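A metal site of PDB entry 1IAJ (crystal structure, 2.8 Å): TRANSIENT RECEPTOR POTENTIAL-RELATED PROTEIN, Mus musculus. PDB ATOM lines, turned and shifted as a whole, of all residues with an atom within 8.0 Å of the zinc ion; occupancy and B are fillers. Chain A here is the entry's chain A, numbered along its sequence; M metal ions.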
ATOM      1  N   GLU A 187      17.152 -13.552 -23.327  1.00  0.00           N
ATOM      2  CA  GLU A 187      17.961 -14.107 -24.383  1.00  0.00           C
ATOM      3  C   GLU A 187      17.235 -14.045 -25.708  1.00  0.00           C
ATOM      4  O   GLU A 187      16.016 -14.155 -25.770  1.00  0.00           O
ATOM      5  CB  GLU A 187      18.349 -15.548 -24.048  1.00  0.00           C
ATOM      6  CG  GLU A 187      17.214 -16.424 -23.559  1.00  0.00           C
ATOM      7  CD  GLU A 187      17.638 -17.867 -23.415  1.00  0.00           C
ATOM      8  OE1 GLU A 187      17.206 -18.714 -24.229  1.00  0.00           O
ATOM      9  OE2 GLU A 187      18.422 -18.158 -22.481  1.00  0.00           O
ATOM     10  N   GLU A 196      22.571 -20.352 -31.217  1.00  0.00           N
ATOM     11  CA  GLU A 196      22.136 -21.488 -30.411  1.00  0.00           C
ATOM     12  C   GLU A 196      23.270 -21.840 -29.449  1.00  0.00           C
ATOM     13  O   GLU A 196      23.066 -21.991 -28.247  1.00  0.00           O
ATOM     14  CB  GLU A 196      21.830 -22.691 -31.301  1.00  0.00           C
ATOM     15  CG  GLU A 196      20.458 -22.649 -31.950  1.00  0.00           C
ATOM     16  CD  GLU A 196      20.018 -24.018 -32.461  1.00  0.00           C
ATOM     17  OE1 GLU A 196      19.155 -24.651 -31.820  1.00  0.00           O
ATOM     18  OE2 GLU A 196      20.524 -24.471 -33.514  1.00  0.00           O
ATOM     19  N   LEU A 199      23.796 -19.309 -26.752  1.00  0.00           N
ATOM     20  CA  LEU A 199      22.796 -19.357 -25.692  1.00  0.00           C
ATOM     21  C   LEU A 199      23.060 -20.548 -24.798  1.00  0.00           C
ATOM     22  O   LEU A 199      22.932 -20.489 -23.574  1.00  0.00           O
ATOM     23  CB  LEU A 199      21.394 -19.438 -26.297  1.00  0.00           C
ATOM     24  CG  LEU A 199      20.883 -18.105 -26.852  1.00  0.00           C
ATOM     25  CD1 LEU A 199      19.375 -18.185 -27.033  1.00  0.00           C
ATOM     26  CD2 LEU A 199      21.232 -16.962 -25.914  1.00  0.00           C
ATOM     27  N   ALA A 200      23.463 -21.645 -25.443  1.00  0.00           N
ATOM     28  CA  ALA A 200      23.783 -22.906 -24.786  1.00  0.00           C
ATOM     29  C   ALA A 200      24.954 -22.785 -23.818  1.00  0.00           C
ATOM     30  O   ALA A 200      24.848 -23.152 -22.641  1.00  0.00           O
ATOM     31  CB  ALA A 200      24.088 -23.958 -25.840  1.00  0.00           C
ATOM     32  N   PHE A 201      26.074 -22.280 -24.313  1.00  0.00           N
ATOM     33  CA  PHE A 201      27.274 -22.114 -23.514  1.00  0.00           C
ATOM     34  C   PHE A 201      26.928 -21.613 -22.122  1.00  0.00           C
ATOM     35  O   PHE A 201      27.335 -22.197 -21.121  1.00  0.00           O
ATOM     36  CB  PHE A 201      28.238 -21.157 -24.208  1.00  0.00           C
ATOM     37  CG  PHE A 201      29.388 -20.709 -23.347  1.00  0.00           C
ATOM     38  CD1 PHE A 201      30.431 -21.577 -23.060  1.00  0.00           C
ATOM     39  CD2 PHE A 201      29.410 -19.425 -22.820  1.00  0.00           C
ATOM     40  CE1 PHE A 201      31.487 -21.168 -22.237  1.00  0.00           C
ATOM     41  CE2 PHE A 201      30.463 -19.003 -22.000  1.00  0.00           C
ATOM     42  CZ  PHE A 201      31.503 -19.869 -21.704  1.00  0.00           C
ATOM     43  N   SER A 202      26.141 -20.544 -22.062  1.00  0.00           N
ATOM     44  CA  SER A 202      25.751 -19.992 -20.780  1.00  0.00           C
ATOM     45  C   SER A 202      25.179 -21.097 -19.910  1.00  0.00           C
ATOM     46  O   SER A 202      25.654 -21.321 -18.786  1.00  0.00           O
ATOM     47  CB  SER A 202      24.712 -18.888 -20.966  1.00  0.00           C
ATOM     48  OG  SER A 202      25.347 -17.627 -20.937  1.00  0.00           O
ATOM     49  N   HIS A 203      24.167 -21.783 -20.422  1.00  0.00           N
ATOM     50  CA  HIS A 203      23.531 -22.892 -19.714  1.00  0.00           C
ATOM     51  C   HIS A 203      24.630 -23.899 -19.318  1.00  0.00           C
ATOM     52  O   HIS A 203      24.690 -24.348 -18.175  1.00  0.00           O
ATOM     53  CB  HIS A 203      22.500 -23.555 -20.645  1.00  0.00           C
ATOM     54  CG  HIS A 203      21.796 -24.737 -20.046  1.00  0.00           C
ATOM     55  ND1 HIS A 203      20.928 -25.510 -20.792  1.00  0.00           N
ATOM     56  CD2 HIS A 203      21.868 -25.230 -18.794  1.00  0.00           C
ATOM     57  CE1 HIS A 203      20.508 -26.458 -19.971  1.00  0.00           C
ATOM     58  NE2 HIS A 203      21.044 -26.328 -18.747  1.00  0.00           N
ATOM     59  N   TRP A 204      25.519 -24.205 -20.260  1.00  0.00           N
ATOM     60  CA  TRP A 204      26.586 -25.165 -20.034  1.00  0.00           C
ATOM     61  C   TRP A 204      27.580 -24.774 -18.961  1.00  0.00           C
ATOM     62  O   TRP A 204      28.206 -25.655 -18.380  1.00  0.00           O
ATOM     63  CB  TRP A 204      27.353 -25.425 -21.329  1.00  0.00           C
ATOM     64  CG  TRP A 204      28.621 -26.223 -21.146  1.00  0.00           C
ATOM     65  CD1 TRP A 204      28.818 -27.521 -21.517  1.00  0.00           C
ATOM     66  CD2 TRP A 204      29.902 -25.734 -20.708  1.00  0.00           C
ATOM     67  NE1 TRP A 204      30.132 -27.872 -21.352  1.00  0.00           N
ATOM     68  CE2 TRP A 204      30.822 -26.795 -20.862  1.00  0.00           C
ATOM     69  CE3 TRP A 204      30.352 -24.508 -20.212  1.00  0.00           C
ATOM     70  CZ2 TRP A 204      32.185 -26.660 -20.538  1.00  0.00           C
ATOM     71  CZ3 TRP A 204      31.706 -24.369 -19.891  1.00  0.00           C
ATOM     72  CH2 TRP A 204      32.607 -25.453 -20.059  1.00  0.00           C
ATOM     73  N   GLU A 207      26.118 -25.765 -15.707  1.00  0.00           N
ATOM     74  CA  GLU A 207      26.201 -27.200 -15.514  1.00  0.00           C
ATOM     75  C   GLU A 207      27.621 -27.605 -15.162  1.00  0.00           C
ATOM     76  O   GLU A 207      27.841 -28.324 -14.194  1.00  0.00           O
ATOM     77  CB  GLU A 207      25.762 -27.925 -16.783  1.00  0.00           C
ATOM     78  CG  GLU A 207      24.315 -27.641 -17.177  1.00  0.00           C
ATOM     79  CD  GLU A 207      23.314 -28.262 -16.222  1.00  0.00           C
ATOM     80  OE1 GLU A 207      22.660 -27.521 -15.454  1.00  0.00           O
ATOM     81  OE2 GLU A 207      23.179 -29.509 -16.236  1.00  0.00           O
ATOM     82  N   PHE A 256      17.606 -16.772 -15.223  1.00  0.00           N
ATOM     83  CA  PHE A 256      18.097 -17.641 -16.285  1.00  0.00           C
ATOM     84  C   PHE A 256      17.519 -19.054 -16.171  1.00  0.00           C
ATOM     85  O   PHE A 256      17.276 -19.714 -17.187  1.00  0.00           O
ATOM     86  CB  PHE A 256      19.636 -17.678 -16.266  1.00  0.00           C
ATOM     87  CG  PHE A 256      20.221 -18.520 -17.363  1.00  0.00           C
ATOM     88  CD1 PHE A 256      20.262 -18.055 -18.678  1.00  0.00           C
ATOM     89  CD2 PHE A 256      20.714 -19.799 -17.105  1.00  0.00           C
ATOM     90  CE1 PHE A 256      20.764 -18.862 -19.714  1.00  0.00           C
ATOM     91  CE2 PHE A 256      21.209 -20.603 -18.122  1.00  0.00           C
ATOM     92  CZ  PHE A 256      21.247 -20.136 -19.428  1.00  0.00           C
ATOM     93  N   HIS A 260      15.690 -19.223 -19.539  1.00  0.00           N
ATOM     94  CA  HIS A 260      16.440 -19.918 -20.592  1.00  0.00           C
ATOM     95  C   HIS A 260      15.709 -21.081 -21.265  1.00  0.00           C
ATOM     96  O   HIS A 260      15.266 -22.023 -20.603  1.00  0.00           O
ATOM     97  CB  HIS A 260      17.780 -20.444 -20.054  1.00  0.00           C
ATOM     98  CG  HIS A 260      18.451 -21.409 -20.981  1.00  0.00           C
ATOM     99  ND1 HIS A 260      18.993 -21.059 -22.204  1.00  0.00           N
ATOM    100  CD2 HIS A 260      18.627 -22.756 -20.878  1.00  0.00           C
ATOM    101  CE1 HIS A 260      19.451 -22.179 -22.782  1.00  0.00           C
ATOM    102  NE2 HIS A 260      19.245 -23.224 -22.006  1.00  0.00           N
ATOM    103  N   HIS A 261      15.591 -21.021 -22.587  1.00  0.00           N
ATOM    104  CA  HIS A 261      14.946 -22.093 -23.331  1.00  0.00           C
ATOM    105  C   HIS A 261      16.031 -22.851 -24.028  1.00  0.00           C
ATOM    106  O   HIS A 261      16.807 -22.291 -24.816  1.00  0.00           O
ATOM    107  CB  HIS A 261      13.990 -21.562 -24.400  1.00  0.00           C
ATOM    108  CG  HIS A 261      12.756 -20.933 -23.842  1.00  0.00           C
ATOM    109  ND1 HIS A 261      12.662 -19.573 -23.617  1.00  0.00           N
ATOM    110  CD2 HIS A 261      11.577 -21.458 -23.462  1.00  0.00           C
ATOM    111  CE1 HIS A 261      11.469 -19.300 -23.112  1.00  0.00           C
ATOM    112  NE2 HIS A 261      10.793 -20.426 -23.018  1.00  0.00           N
ATOM    113  N   CYS A 262      16.087 -24.146 -23.761  1.00  0.00           N
ATOM    114  CA  CYS A 262      17.118 -24.969 -24.368  1.00  0.00           C
ATOM    115  C   CYS A 262      16.828 -25.105 -25.837  1.00  0.00           C
ATOM    116  O   CYS A 262      15.675 -25.184 -26.246  1.00  0.00           O
ATOM    117  CB  CYS A 262      17.187 -26.342 -23.686  1.00  0.00           C
ATOM    118  SG  CYS A 262      17.909 -26.262 -22.010  1.00  0.00           S
ATOM    119  N   ASN A 263      17.888 -25.110 -26.630  1.00  0.00           N
ATOM    120  CA  ASN A 263      17.789 -25.240 -28.074  1.00  0.00           C
ATOM    121  C   ASN A 263      18.391 -26.575 -28.423  1.00  0.00           C
ATOM    122  O   ASN A 263      18.774 -27.337 -27.540  1.00  0.00           O
ATOM    123  CB  ASN A 263      18.566 -24.131 -28.764  1.00  0.00           C
ATOM    124  CG  ASN A 263      19.773 -23.680 -27.969  1.00  0.00           C
ATOM    125  OD1 ASN A 263      20.871 -24.221 -28.118  1.00  0.00           O
ATOM    126  ND2 ASN A 263      19.573 -22.670 -27.118  1.00  0.00           N
ATOM    127  N   SER A 264      18.494 -26.859 -29.714  1.00  0.00           N
ATOM    128  CA  SER A 264      19.049 -28.129 -30.178  1.00  0.00           C
ATOM    129  C   SER A 264      20.485 -28.294 -29.690  1.00  0.00           C
ATOM    130  O   SER A 264      20.998 -29.407 -29.592  1.00  0.00           O
ATOM    131  CB  SER A 264      19.017 -28.191 -31.707  1.00  0.00           C
ATOM    132  OG  SER A 264      20.171 -28.834 -32.215  1.00  0.00           O
ATOM    133  N   CYS A 265      21.142 -27.169 -29.392  1.00  0.00           N
ATOM    134  CA  CYS A 265      22.512 -27.216 -28.937  1.00  0.00           C
ATOM    135  C   CYS A 265      22.582 -27.713 -27.523  1.00  0.00           C
ATOM    136  O   CYS A 265      23.330 -28.653 -27.254  1.00  0.00           O
ATOM    137  CB  CYS A 265      23.163 -25.844 -29.071  1.00  0.00           C
ATOM    138  SG  CYS A 265      23.639 -25.569 -30.789  1.00  0.00           S
ATOM    139  N   CYS A 266      21.805 -27.101 -26.627  1.00  0.00           N
ATOM    140  CA  CYS A 266      21.779 -27.553 -25.245  1.00  0.00           C
ATOM    141  C   CYS A 266      21.680 -29.096 -25.281  1.00  0.00           C
ATOM    142  O   CYS A 266      22.341 -29.785 -24.505  1.00  0.00           O
ATOM    143  CB  CYS A 266      20.587 -26.953 -24.516  1.00  0.00           C
ATOM    144  SG  CYS A 266      20.625 -25.146 -24.472  1.00  0.00           S
ATOM    145  N   ARG A 267      20.873 -29.622 -26.199  1.00  0.00           N
ATOM    146  CA  ARG A 267      20.714 -31.058 -26.351  1.00  0.00           C
ATOM    147  C   ARG A 267      22.005 -31.722 -26.861  1.00  0.00           C
ATOM    148  O   ARG A 267      22.477 -32.710 -26.294  1.00  0.00           O
ATOM    149  CB  ARG A 267      19.577 -31.383 -27.325  1.00  0.00           C
ATOM    150  CG  ARG A 267      18.172 -31.349 -26.693  1.00  0.00           C
ATOM    151  CD  ARG A 267      17.070 -30.933 -27.697  1.00  0.00           C
ATOM    152  NE  ARG A 267      16.660 -29.530 -27.517  1.00  0.00           N
ATOM    153  CZ  ARG A 267      15.627 -29.136 -26.771  1.00  0.00           C
ATOM    154  NH1 ARG A 267      14.883 -30.033 -26.128  1.00  0.00           N
ATOM    155  NH2 ARG A 267      15.341 -27.849 -26.656  1.00  0.00           N
ATOM    156  N   LEU A 269      24.780 -30.958 -26.345  1.00  0.00           N
ATOM    157  CA  LEU A 269      25.710 -30.935 -25.221  1.00  0.00           C
ATOM    158  C   LEU A 269      25.165 -31.662 -24.008  1.00  0.00           C
ATOM    159  O   LEU A 269      25.786 -31.657 -22.938  1.00  0.00           O
ATOM    160  CB  LEU A 269      26.010 -29.507 -24.791  1.00  0.00           C
ATOM    161  CG  LEU A 269      26.617 -28.567 -25.813  1.00  0.00           C
ATOM    162  CD1 LEU A 269      26.916 -27.249 -25.139  1.00  0.00           C
ATOM    163  CD2 LEU A 269      27.871 -29.184 -26.399  1.00  0.00           C
ATOM    164  N   LYS A 270      23.978 -32.236 -24.161  1.00  0.00           N
ATOM    165  CA  LYS A 270      23.358 -32.975 -23.071  1.00  0.00           C
ATOM    166  C   LYS A 270      23.203 -32.118 -21.833  1.00  0.00           C
ATOM    167  O   LYS A 270      23.581 -32.527 -20.734  1.00  0.00           O
ATOM    168  CB  LYS A 270      24.206 -34.205 -22.737  1.00  0.00           C
ATOM    169  CG  LYS A 270      24.828 -34.868 -23.959  1.00  0.00           C
ATOM    170  CD  LYS A 270      23.782 -35.582 -24.812  1.00  0.00           C
ATOM    171  CE  LYS A 270      23.756 -37.084 -24.550  1.00  0.00           C
ATOM    172  NZ  LYS A 270      25.103 -37.643 -24.207  1.00  0.00           N
ATOM    173  N   LEU A 271      22.652 -30.924 -21.990  1.00  0.00           N
ATOM    174  CA  LEU A 271      22.477 -30.041 -20.839  1.00  0.00           C
ATOM    175  C   LEU A 271      21.111 -30.181 -20.184  1.00  0.00           C
ATOM    176  O   LEU A 271      20.106 -29.729 -20.730  1.00  0.00           O
ATOM    177  CB  LEU A 271      22.700 -28.579 -21.229  1.00  0.00           C
ATOM    178  CG  LEU A 271      24.127 -28.139 -21.581  1.00  0.00           C
ATOM    179  CD1 LEU A 271      24.165 -26.641 -21.548  1.00  0.00           C
ATOM    180  CD2 LEU A 271      25.154 -28.718 -20.618  1.00  0.00           C
ATOM    181  N   PRO A 272      21.064 -30.822 -19.024  1.00  0.00           N
ATOM    182  CA  PRO A 272      19.829 -31.039 -18.266  1.00  0.00           C
ATOM    183  C   PRO A 272      18.933 -29.803 -18.242  1.00  0.00           C
ATOM    184  O   PRO A 272      19.398 -28.671 -18.358  1.00  0.00           O
ATOM    185  CB  PRO A 272      20.341 -31.372 -16.874  1.00  0.00           C
ATOM    186  CG  PRO A 272      21.620 -32.082 -17.143  1.00  0.00           C
ATOM    187  CD  PRO A 272      22.226 -31.446 -18.361  1.00  0.00           C
ATOM    188  N   ASP A 273      17.633 -30.023 -18.077  1.00  0.00           N
ATOM    189  CA  ASP A 273      16.688 -28.909 -18.048  1.00  0.00           C
ATOM    190  C   ASP A 273      16.784 -28.034 -16.821  1.00  0.00           C
ATOM    191  O   ASP A 273      16.303 -28.379 -15.749  1.00  0.00           O
ATOM    192  CB  ASP A 273      15.253 -29.411 -18.194  1.00  0.00           C
ATOM    193  CG  ASP A 273      14.381 -28.398 -18.886  1.00  0.00           C
ATOM    194  OD1 ASP A 273      13.926 -27.434 -18.216  1.00  0.00           O
ATOM    195  OD2 ASP A 273      14.171 -28.553 -20.118  1.00  0.00           O
ATOM    196  N   LEU A 274      17.396 -26.869 -16.998  1.00  0.00           N
ATOM    197  CA  LEU A 274      17.596 -25.921 -15.929  1.00  0.00           C
ATOM    198  C   LEU A 274      16.477 -25.798 -14.908  1.00  0.00           C
ATOM    199  O   LEU A 274      16.752 -25.518 -13.740  1.00  0.00           O
ATOM    200  CB  LEU A 274      17.867 -24.550 -16.512  1.00  0.00           C
ATOM    201  CG  LEU A 274      19.201 -24.012 -16.020  1.00  0.00           C
ATOM    202  CD1 LEU A 274      20.273 -25.067 -16.196  1.00  0.00           C
ATOM    203  CD2 LEU A 274      19.532 -22.785 -16.782  1.00  0.00           C
HETATM  204 ZN    ZN M   1      19.777 -25.023 -22.440  1.00  0.00          ZN
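The backbone carbonyl oxygen (O) of Pro 272 is in hydrogen-bond range of a ring nitrogen (NE2) of His 203, 2.9 Å away. N of Leu 271 is in hydrogen-bond range of O of Cys 266 (2.8 Å). The backbone NH of Cys 266 lies within hydrogen-bond range of the side-chain amide oxygen of Asn 263 (3.4 Å). The backbone carbonyl oxygen (O) of Cys 262 lies within hydrogen-bond range of the guanidinium group (NH2) of Arg 267, at 2.7 Å. ND1 of His 260 lies within hydrogen-bond range of OE2 of Glu 187, 3.0 Å away.
Of the 24 residues printed, 4 come within 4 Å of the zinc ion.
The zinc ion is bound by NE2 of His 260 (1.9 Å), ND1 of His 203 (2.1 Å), SG of Cys 266 (2.2 Å) and SG of Cys 262 (2.3 Å).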
